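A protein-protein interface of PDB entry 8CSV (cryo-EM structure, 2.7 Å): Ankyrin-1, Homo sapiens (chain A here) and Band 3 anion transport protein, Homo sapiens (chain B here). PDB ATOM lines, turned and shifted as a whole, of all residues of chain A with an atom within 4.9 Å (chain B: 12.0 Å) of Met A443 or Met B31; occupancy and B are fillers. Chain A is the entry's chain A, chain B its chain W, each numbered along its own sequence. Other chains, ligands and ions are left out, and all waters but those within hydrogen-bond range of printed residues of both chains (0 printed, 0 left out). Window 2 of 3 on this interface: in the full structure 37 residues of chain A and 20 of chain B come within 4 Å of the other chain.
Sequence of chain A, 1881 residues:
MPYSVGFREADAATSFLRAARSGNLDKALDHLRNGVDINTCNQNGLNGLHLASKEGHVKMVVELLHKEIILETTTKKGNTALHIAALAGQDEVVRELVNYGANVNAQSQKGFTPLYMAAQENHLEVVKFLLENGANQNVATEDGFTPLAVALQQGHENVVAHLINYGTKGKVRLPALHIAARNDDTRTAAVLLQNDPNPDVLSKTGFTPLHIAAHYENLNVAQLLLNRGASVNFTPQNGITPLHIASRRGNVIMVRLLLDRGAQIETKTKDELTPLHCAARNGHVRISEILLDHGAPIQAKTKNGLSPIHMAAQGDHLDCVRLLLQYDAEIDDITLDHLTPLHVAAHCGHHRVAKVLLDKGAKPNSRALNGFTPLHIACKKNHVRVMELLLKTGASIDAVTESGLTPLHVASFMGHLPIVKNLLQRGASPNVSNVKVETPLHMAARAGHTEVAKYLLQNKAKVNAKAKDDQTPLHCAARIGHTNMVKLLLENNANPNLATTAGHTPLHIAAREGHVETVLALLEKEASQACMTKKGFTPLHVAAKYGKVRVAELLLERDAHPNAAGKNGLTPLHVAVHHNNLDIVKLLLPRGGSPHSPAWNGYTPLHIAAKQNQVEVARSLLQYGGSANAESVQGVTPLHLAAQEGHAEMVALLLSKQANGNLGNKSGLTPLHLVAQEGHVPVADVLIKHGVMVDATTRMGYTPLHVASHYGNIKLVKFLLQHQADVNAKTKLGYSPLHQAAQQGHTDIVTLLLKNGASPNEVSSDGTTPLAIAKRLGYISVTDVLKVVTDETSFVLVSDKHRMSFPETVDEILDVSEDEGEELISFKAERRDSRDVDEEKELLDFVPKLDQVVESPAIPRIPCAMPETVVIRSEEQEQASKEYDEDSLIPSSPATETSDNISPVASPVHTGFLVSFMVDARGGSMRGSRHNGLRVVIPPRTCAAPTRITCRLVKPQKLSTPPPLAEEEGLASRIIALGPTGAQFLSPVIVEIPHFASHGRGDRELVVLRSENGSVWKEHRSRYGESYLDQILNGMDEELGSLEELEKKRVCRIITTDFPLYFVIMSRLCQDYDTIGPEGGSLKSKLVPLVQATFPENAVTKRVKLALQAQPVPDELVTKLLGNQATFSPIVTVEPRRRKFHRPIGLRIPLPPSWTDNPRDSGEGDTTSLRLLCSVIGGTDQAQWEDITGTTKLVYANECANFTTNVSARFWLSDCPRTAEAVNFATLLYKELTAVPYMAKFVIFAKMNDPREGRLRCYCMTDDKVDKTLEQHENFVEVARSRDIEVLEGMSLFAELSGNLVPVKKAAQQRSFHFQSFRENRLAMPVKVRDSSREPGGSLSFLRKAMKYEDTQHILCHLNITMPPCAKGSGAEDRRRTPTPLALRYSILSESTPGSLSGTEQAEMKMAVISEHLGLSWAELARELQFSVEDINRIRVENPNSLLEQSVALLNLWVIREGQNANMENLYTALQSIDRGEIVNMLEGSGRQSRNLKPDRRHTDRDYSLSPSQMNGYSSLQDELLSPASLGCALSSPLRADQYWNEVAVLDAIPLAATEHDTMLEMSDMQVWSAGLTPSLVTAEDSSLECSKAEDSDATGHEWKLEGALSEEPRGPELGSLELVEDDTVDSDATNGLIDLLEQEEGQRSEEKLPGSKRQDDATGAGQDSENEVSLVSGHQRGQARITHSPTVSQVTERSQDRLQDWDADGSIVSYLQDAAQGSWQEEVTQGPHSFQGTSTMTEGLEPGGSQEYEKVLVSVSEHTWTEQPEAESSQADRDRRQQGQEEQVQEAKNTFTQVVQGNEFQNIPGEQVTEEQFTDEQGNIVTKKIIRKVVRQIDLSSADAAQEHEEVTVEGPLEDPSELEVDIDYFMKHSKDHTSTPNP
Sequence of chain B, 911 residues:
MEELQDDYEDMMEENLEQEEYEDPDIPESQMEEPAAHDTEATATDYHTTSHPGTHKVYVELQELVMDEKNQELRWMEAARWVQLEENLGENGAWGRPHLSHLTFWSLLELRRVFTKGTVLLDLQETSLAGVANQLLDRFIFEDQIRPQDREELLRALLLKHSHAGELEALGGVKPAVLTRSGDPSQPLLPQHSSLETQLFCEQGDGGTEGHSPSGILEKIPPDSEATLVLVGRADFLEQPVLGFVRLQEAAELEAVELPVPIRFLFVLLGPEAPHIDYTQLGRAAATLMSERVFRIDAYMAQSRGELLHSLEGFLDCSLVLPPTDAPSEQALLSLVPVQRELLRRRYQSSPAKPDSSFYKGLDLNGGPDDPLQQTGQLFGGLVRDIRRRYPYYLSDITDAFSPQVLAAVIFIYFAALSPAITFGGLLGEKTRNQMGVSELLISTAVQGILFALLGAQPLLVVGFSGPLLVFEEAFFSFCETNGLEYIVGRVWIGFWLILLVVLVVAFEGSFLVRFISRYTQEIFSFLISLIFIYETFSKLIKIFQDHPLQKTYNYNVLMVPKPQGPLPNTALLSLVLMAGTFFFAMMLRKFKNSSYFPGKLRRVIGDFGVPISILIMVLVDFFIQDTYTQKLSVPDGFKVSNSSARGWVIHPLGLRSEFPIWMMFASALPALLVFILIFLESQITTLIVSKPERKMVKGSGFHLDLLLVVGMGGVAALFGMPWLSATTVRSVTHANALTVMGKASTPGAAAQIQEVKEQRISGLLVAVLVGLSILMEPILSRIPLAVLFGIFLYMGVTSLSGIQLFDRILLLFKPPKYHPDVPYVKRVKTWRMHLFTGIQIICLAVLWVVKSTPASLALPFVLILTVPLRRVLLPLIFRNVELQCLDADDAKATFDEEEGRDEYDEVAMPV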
ATOM      1  N   PHE A 372       7.760  -0.131   0.811  1.00  0.00           N
ATOM      2  CA  PHE A 372       7.893  -0.164   2.259  1.00  0.00           C
ATOM      3  C   PHE A 372       9.195   0.496   2.697  1.00  0.00           C
ATOM      4  O   PHE A 372      10.266   0.221   2.151  1.00  0.00           O
ATOM      5  CB  PHE A 372       7.840  -1.604   2.766  1.00  0.00           C
ATOM      6  CG  PHE A 372       6.450  -2.157   2.880  1.00  0.00           C
ATOM      7  CD1 PHE A 372       5.745  -2.539   1.751  1.00  0.00           C
ATOM      8  CD2 PHE A 372       5.850  -2.306   4.118  1.00  0.00           C
ATOM      9  CE1 PHE A 372       4.466  -3.050   1.857  1.00  0.00           C
ATOM     10  CE2 PHE A 372       4.573  -2.815   4.231  1.00  0.00           C
ATOM     11  CZ  PHE A 372       3.880  -3.188   3.099  1.00  0.00           C
ATOM     12  N   LYS A 380       5.265  -2.961  11.342  1.00  0.00           N
ATOM     13  CA  LYS A 380       4.619  -4.242  11.065  1.00  0.00           C
ATOM     14  C   LYS A 380       5.007  -5.297  12.092  1.00  0.00           C
ATOM     15  O   LYS A 380       4.165  -6.096  12.516  1.00  0.00           O
ATOM     16  CB  LYS A 380       4.978  -4.721   9.659  1.00  0.00           C
ATOM     17  CG  LYS A 380       4.241  -5.981   9.245  1.00  0.00           C
ATOM     18  CD  LYS A 380       4.528  -6.346   7.803  1.00  0.00           C
ATOM     19  CE  LYS A 380       3.766  -7.593   7.395  1.00  0.00           C
ATOM     20  NZ  LYS A 380       4.239  -8.800   8.126  1.00  0.00           N
ATOM     21  N   LEU A 405      -0.252   2.667   1.991  1.00  0.00           N
ATOM     22  CA  LEU A 405      -0.259   2.301   3.402  1.00  0.00           C
ATOM     23  C   LEU A 405       0.718   3.172   4.183  1.00  0.00           C
ATOM     24  O   LEU A 405       1.912   3.214   3.868  1.00  0.00           O
ATOM     25  CB  LEU A 405       0.099   0.827   3.563  1.00  0.00           C
ATOM     26  CG  LEU A 405      -0.899  -0.210   3.052  1.00  0.00           C
ATOM     27  CD1 LEU A 405      -0.216  -1.554   2.879  1.00  0.00           C
ATOM     28  CD2 LEU A 405      -2.073  -0.331   4.005  1.00  0.00           C
ATOM     29  N   HIS A 409      -1.431   2.701   9.209  1.00  0.00           N
ATOM     30  CA  HIS A 409      -2.208   1.648   8.558  1.00  0.00           C
ATOM     31  C   HIS A 409      -1.692   0.266   8.935  1.00  0.00           C
ATOM     32  O   HIS A 409      -2.465  -0.604   9.356  1.00  0.00           O
ATOM     33  CB  HIS A 409      -2.152   1.812   7.039  1.00  0.00           C
ATOM     34  CG  HIS A 409      -3.233   2.673   6.471  1.00  0.00           C
ATOM     35  ND1 HIS A 409      -2.972   3.733   5.630  1.00  0.00           N
ATOM     36  CD2 HIS A 409      -4.580   2.612   6.592  1.00  0.00           C
ATOM     37  CE1 HIS A 409      -4.109   4.300   5.272  1.00  0.00           C
ATOM     38  NE2 HIS A 409      -5.100   3.639   5.840  1.00  0.00           N
ATOM     39  N   VAL A 410      -0.383   0.053   8.787  1.00  0.00           N
ATOM     40  CA  VAL A 410       0.211  -1.251   9.053  1.00  0.00           C
ATOM     41  C   VAL A 410       0.081  -1.611  10.526  1.00  0.00           C
ATOM     42  O   VAL A 410      -0.250  -2.751  10.872  1.00  0.00           O
ATOM     43  CB  VAL A 410       1.680  -1.259   8.595  1.00  0.00           C
ATOM     44  CG1 VAL A 410       2.255  -2.644   8.720  1.00  0.00           C
ATOM     45  CG2 VAL A 410       1.791  -0.759   7.165  1.00  0.00           C
ATOM     46  N   SER A 412      -2.171  -0.536  12.715  1.00  0.00           N
ATOM     47  CA  SER A 412      -3.561  -0.812  13.059  1.00  0.00           C
ATOM     48  C   SER A 412      -4.016  -2.153  12.503  1.00  0.00           C
ATOM     49  O   SER A 412      -4.770  -2.878  13.161  1.00  0.00           O
ATOM     50  CB  SER A 412      -4.462   0.312  12.553  1.00  0.00           C
ATOM     51  OG  SER A 412      -4.143   1.538  13.183  1.00  0.00           O
ATOM     52  N   PHE A 413      -3.583  -2.499  11.287  1.00  0.00           N
ATOM     53  CA  PHE A 413      -3.961  -3.790  10.726  1.00  0.00           C
ATOM     54  C   PHE A 413      -3.321  -4.939  11.496  1.00  0.00           C
ATOM     55  O   PHE A 413      -3.958  -5.976  11.716  1.00  0.00           O
ATOM     56  CB  PHE A 413      -3.587  -3.860   9.248  1.00  0.00           C
ATOM     57  CG  PHE A 413      -3.905  -5.180   8.610  1.00  0.00           C
ATOM     58  CD1 PHE A 413      -5.215  -5.617   8.511  1.00  0.00           C
ATOM     59  CD2 PHE A 413      -2.895  -5.988   8.117  1.00  0.00           C
ATOM     60  CE1 PHE A 413      -5.513  -6.832   7.933  1.00  0.00           C
ATOM     61  CE2 PHE A 413      -3.187  -7.203   7.534  1.00  0.00           C
ATOM     62  CZ  PHE A 413      -4.496  -7.627   7.441  1.00  0.00           C
ATOM     63  N   MET A 414      -2.066  -4.777  11.914  1.00  0.00           N
ATOM     64  CA  MET A 414      -1.378  -5.826  12.653  1.00  0.00           C
ATOM     65  C   MET A 414      -1.796  -5.902  14.116  1.00  0.00           C
ATOM     66  O   MET A 414      -1.481  -6.895  14.778  1.00  0.00           O
ATOM     67  CB  MET A 414       0.135  -5.627  12.560  1.00  0.00           C
ATOM     68  CG  MET A 414       0.700  -5.844  11.168  1.00  0.00           C
ATOM     69  SD  MET A 414       0.364  -7.498  10.538  1.00  0.00           S
ATOM     70  CE  MET A 414       1.165  -8.501  11.786  1.00  0.00           C
ATOM     71  N   GLU A 438      -9.495   3.024   2.258  1.00  0.00           N
ATOM     72  CA  GLU A 438      -9.641   2.537   3.621  1.00  0.00           C
ATOM     73  C   GLU A 438      -8.717   3.283   4.576  1.00  0.00           C
ATOM     74  O   GLU A 438      -7.566   3.582   4.249  1.00  0.00           O
ATOM     75  CB  GLU A 438      -9.346   1.039   3.679  1.00  0.00           C
ATOM     76  CG  GLU A 438     -10.163   0.206   2.709  1.00  0.00           C
ATOM     77  CD  GLU A 438      -9.791  -1.261   2.751  1.00  0.00           C
ATOM     78  OE1 GLU A 438      -8.807  -1.605   3.439  1.00  0.00           O
ATOM     79  OE2 GLU A 438     -10.483  -2.071   2.098  1.00  0.00           O
ATOM     80  N   THR A 439      -9.229   3.573   5.760  1.00  0.00           N
ATOM     81  CA  THR A 439      -8.492   4.275   6.800  1.00  0.00           C
ATOM     82  C   THR A 439      -7.884   3.272   7.770  1.00  0.00           C
ATOM     83  O   THR A 439      -8.148   2.070   7.686  1.00  0.00           O
ATOM     84  CB  THR A 439      -9.432   5.248   7.511  1.00  0.00           C
ATOM     85  OG1 THR A 439     -10.517   4.525   8.102  1.00  0.00           O
ATOM     86  CG2 THR A 439      -9.985   6.260   6.522  1.00  0.00           C
ATOM     87  N   PRO A 440      -7.020   3.721   8.693  1.00  0.00           N
ATOM     88  CA  PRO A 440      -6.561   2.803   9.752  1.00  0.00           C
ATOM     89  C   PRO A 440      -7.690   2.217  10.581  1.00  0.00           C
ATOM     90  O   PRO A 440      -7.568   1.092  11.079  1.00  0.00           O
ATOM     91  CB  PRO A 440      -5.636   3.689  10.594  1.00  0.00           C
ATOM     92  CG  PRO A 440      -5.083   4.647   9.624  1.00  0.00           C
ATOM     93  CD  PRO A 440      -6.187   4.939   8.646  1.00  0.00           C
ATOM     94  N   LEU A 441      -8.789   2.956  10.749  1.00  0.00           N
ATOM     95  CA  LEU A 441      -9.954   2.401  11.429  1.00  0.00           C
ATOM     96  C   LEU A 441     -10.549   1.241  10.640  1.00  0.00           C
ATOM     97  O   LEU A 441     -10.997   0.250  11.227  1.00  0.00           O
ATOM     98  CB  LEU A 441     -10.997   3.492  11.657  1.00  0.00           C
ATOM     99  CG  LEU A 441     -12.268   3.073  12.393  1.00  0.00           C
ATOM    100  CD1 LEU A 441     -11.932   2.435  13.730  1.00  0.00           C
ATOM    101  CD2 LEU A 441     -13.182   4.269  12.582  1.00  0.00           C
ATOM    102  N   HIS A 442     -10.562   1.344   9.307  1.00  0.00           N
ATOM    103  CA  HIS A 442     -11.016   0.228   8.482  1.00  0.00           C
ATOM    104  C   HIS A 442     -10.134  -0.997   8.677  1.00  0.00           C
ATOM    105  O   HIS A 442     -10.635  -2.123   8.773  1.00  0.00           O
ATOM    106  CB  HIS A 442     -11.039   0.625   7.006  1.00  0.00           C
ATOM    107  CG  HIS A 442     -12.141   1.570   6.644  1.00  0.00           C
ATOM    108  ND1 HIS A 442     -12.066   2.926   6.875  1.00  0.00           N
ATOM    109  CD2 HIS A 442     -13.342   1.355   6.056  1.00  0.00           C
ATOM    110  CE1 HIS A 442     -13.175   3.505   6.450  1.00  0.00           C
ATOM    111  NE2 HIS A 442     -13.965   2.574   5.949  1.00  0.00           N
ATOM    112  N   MET A 443      -8.814  -0.798   8.728  1.00  0.00           N
ATOM    113  CA  MET A 443      -7.901  -1.919   8.931  1.00  0.00           C
ATOM    114  C   MET A 443      -8.092  -2.543  10.309  1.00  0.00           C
ATOM    115  O   MET A 443      -8.040  -3.769  10.456  1.00  0.00           O
ATOM    116  CB  MET A 443      -6.455  -1.458   8.745  1.00  0.00           C
ATOM    117  CG  MET A 443      -6.231  -0.588   7.522  1.00  0.00           C
ATOM    118  SD  MET A 443      -6.381  -1.470   5.957  1.00  0.00           S
ATOM    119  CE  MET A 443      -4.811  -2.325   5.899  1.00  0.00           C
ATOM    120  N   ALA A 444      -8.309  -1.713  11.331  1.00  0.00           N
ATOM    121  CA  ALA A 444      -8.549  -2.235  12.673  1.00  0.00           C
ATOM    122  C   ALA A 444      -9.872  -2.986  12.762  1.00  0.00           C
ATOM    123  O   ALA A 444      -9.961  -3.996  13.468  1.00  0.00           O
ATOM    124  CB  ALA A 444      -8.515  -1.098  13.693  1.00  0.00           C
ATOM    125  N   ALA A 445     -10.907  -2.511  12.067  1.00  0.00           N
ATOM    126  CA  ALA A 445     -12.204  -3.174  12.104  1.00  0.00           C
ATOM    127  C   ALA A 445     -12.225  -4.449  11.271  1.00  0.00           C
ATOM    128  O   ALA A 445     -12.965  -5.382  11.599  1.00  0.00           O
ATOM    129  CB  ALA A 445     -13.296  -2.218  11.626  1.00  0.00           C
ATOM    130  N   ARG A 446     -11.434  -4.514  10.201  1.00  0.00           N
ATOM    131  CA  ARG A 446     -11.391  -5.708   9.368  1.00  0.00           C
ATOM    132  C   ARG A 446     -10.547  -6.820   9.974  1.00  0.00           C
ATOM    133  O   ARG A 446     -10.565  -7.942   9.455  1.00  0.00           O
ATOM    134  CB  ARG A 446     -10.860  -5.363   7.974  1.00  0.00           C
ATOM    135  CG  ARG A 446     -11.448  -6.219   6.866  1.00  0.00           C
ATOM    136  CD  ARG A 446     -10.816  -5.916   5.519  1.00  0.00           C
ATOM    137  NE  ARG A 446      -9.595  -6.683   5.301  1.00  0.00           N
ATOM    138  CZ  ARG A 446      -8.370  -6.221   5.508  1.00  0.00           C
ATOM    139  NH1 ARG A 446      -8.160  -4.990   5.945  1.00  0.00           N
ATOM    140  NH2 ARG A 446      -7.330  -7.012   5.265  1.00  0.00           N
ATOM    141  N   ALA A 447      -9.810  -6.540  11.048  1.00  0.00           N
ATOM    142  CA  ALA A 447      -9.001  -7.543  11.722  1.00  0.00           C
ATOM    143  C   ALA A 447      -9.430  -7.785  13.161  1.00  0.00           C
ATOM    144  O   ALA A 447      -8.786  -8.577  13.858  1.00  0.00           O
ATOM    145  CB  ALA A 447      -7.519  -7.146  11.688  1.00  0.00           C
ATOM    146  N   ILE B  26      14.593 -14.693   1.016  1.00  0.00           N
ATOM    147  CA  ILE B  26      14.479 -13.252   1.214  1.00  0.00           C
ATOM    148  C   ILE B  26      13.178 -12.991   1.963  1.00  0.00           C
ATOM    149  O   ILE B  26      12.095 -13.204   1.400  1.00  0.00           O
ATOM    150  CB  ILE B  26      14.512 -12.489  -0.120  1.00  0.00           C
ATOM    151  N   PRO B  27      13.226 -12.548   3.222  1.00  0.00           N
ATOM    152  CA  PRO B  27      11.983 -12.319   3.971  1.00  0.00           C
ATOM    153  C   PRO B  27      11.189 -11.145   3.426  1.00  0.00           C
ATOM    154  O   PRO B  27      11.591  -9.987   3.578  1.00  0.00           O
ATOM    155  CB  PRO B  27      12.475 -12.048   5.400  1.00  0.00           C
ATOM    156  CG  PRO B  27      13.871 -12.600   5.445  1.00  0.00           C
ATOM    157  CD  PRO B  27      14.418 -12.391   4.070  1.00  0.00           C
ATOM    158  N   GLU B  28      10.057 -11.436   2.785  1.00  0.00           N
ATOM    159  CA  GLU B  28       9.191 -10.404   2.226  1.00  0.00           C
ATOM    160  C   GLU B  28       8.054 -10.052   3.179  1.00  0.00           C
ATOM    161  O   GLU B  28       7.907  -8.889   3.568  1.00  0.00           O
ATOM    162  CB  GLU B  28       8.637 -10.859   0.870  1.00  0.00           C
ATOM    163  N   SER B  29       7.251 -11.049   3.564  1.00  0.00           N
ATOM    164  CA  SER B  29       6.156 -10.898   4.522  1.00  0.00           C
ATOM    165  C   SER B  29       5.169  -9.820   4.057  1.00  0.00           C
ATOM    166  O   SER B  29       5.006  -8.768   4.676  1.00  0.00           O
ATOM    167  CB  SER B  29       6.692 -10.597   5.928  1.00  0.00           C
ATOM    168  N   GLN B  30       4.541 -10.105   2.918  1.00  0.00           N
ATOM    169  CA  GLN B  30       3.540  -9.201   2.369  1.00  0.00           C
ATOM    170  C   GLN B  30       2.358  -9.079   3.323  1.00  0.00           C
ATOM    171  O   GLN B  30       1.821 -10.082   3.800  1.00  0.00           O
ATOM    172  CB  GLN B  30       3.071  -9.697   1.001  1.00  0.00           C
ATOM    173  N   MET B  31       1.952  -7.837   3.598  1.00  0.00           N
ATOM    174  CA  MET B  31       0.888  -7.594   4.564  1.00  0.00           C
ATOM    175  C   MET B  31      -0.493  -7.908   4.003  1.00  0.00           C
ATOM    176  O   MET B  31      -1.437  -8.082   4.780  1.00  0.00           O
ATOM    177  CB  MET B  31       0.937  -6.141   5.041  1.00  0.00           C
ATOM    178  CG  MET B  31       0.251  -5.898   6.376  1.00  0.00           C
ATOM    179  SD  MET B  31      -0.238  -4.180   6.600  1.00  0.00           S
ATOM    180  CE  MET B  31      -1.496  -4.024   5.334  1.00  0.00           C
ATOM    181  N   GLU B  32      -0.631  -7.980   2.680  1.00  0.00           N
ATOM    182  CA  GLU B  32      -1.933  -8.223   2.070  1.00  0.00           C
ATOM    183  C   GLU B  32      -2.440  -9.617   2.417  1.00  0.00           C
ATOM    184  O   GLU B  32      -1.691 -10.597   2.369  1.00  0.00           O
ATOM    185  CB  GLU B  32      -1.842  -8.056   0.553  1.00  0.00           C
ATOM    186  N   GLU B  33      -3.720  -9.701   2.768  1.00  0.00           N
ATOM    187  CA  GLU B  33      -4.335 -10.971   3.134  1.00  0.00           C
ATOM    188  C   GLU B  33      -4.924 -11.663   1.910  1.00  0.00           C
ATOM    189  O   GLU B  33      -4.940 -11.102   0.815  1.00  0.00           O
ATOM    190  CB  GLU B  33      -5.419 -10.755   4.192  1.00  0.00           C
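Among the printed residues, merely in contact across the chains: Lys A380 with Ser B29, Lys A380 with Met B31, Leu A405 with Met B31, Val A410 with Met B31, Phe A413 with Met B31 and Met A443 with Met B31.
Printed residues of chain A that touch a printed residue of chain B: Lys A380, Leu A405, Val A410, Phe A413 and Met A443.
Hydrophobic or aromatic side chains of chain A that line the printed part of chain B: Leu A405, Val A410, Phe A413 and Met A443.
Hydrophobic or aromatic side chains of chain B that line the printed part of chain A: Met B31.
Among the printed residues, no Asp or Glu carboxylate lies within 4 Å of a Lys or Arg side-chain nitrogen of the other chain.
Phe A372 touches none of the printed residues of chain B.
Printed residues of chain B within 4 Å of Leu A405: Met B31.
His A409 touches none of the printed residues of chain B.
Of the printed residues of chain B, Val A410 touches Met B31 (3.6 Å).
No residue of chain B comes within 4 Å of Ser A412.
Glu A438 touches none of the printed residues of chain B.
No residue of chain B comes within 4 Å of Thr A439.
No residue of chain B comes within 4 Å of Pro A440.
No residue of chain B comes within 4 Å of His A442.
Printed residues of chain B within 4 Å of Met A443: Met B31 (3.8 Å).
No residue of chain B comes within 4 Å of Ala A445.
No residue of chain B comes within 4 Å of Arg A446.
Of the printed residues of chain A, Ser B29 touches Lys A380 (3.2 Å).
Of chain A, only Lys A380 (3.96 Å), Leu A405 (3.7 Å), Val A410 (3.6 Å), Phe A413 (3.4 Å) and Met A443 (3.8 Å) come within 4 Å of Met B31.
The nearest residue of chain B that does not touch Met A443 is Glu B32 (7.6 Å).
The nearest residue of chain A that does not touch Met B31 is Met A414 (4.5 Å).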
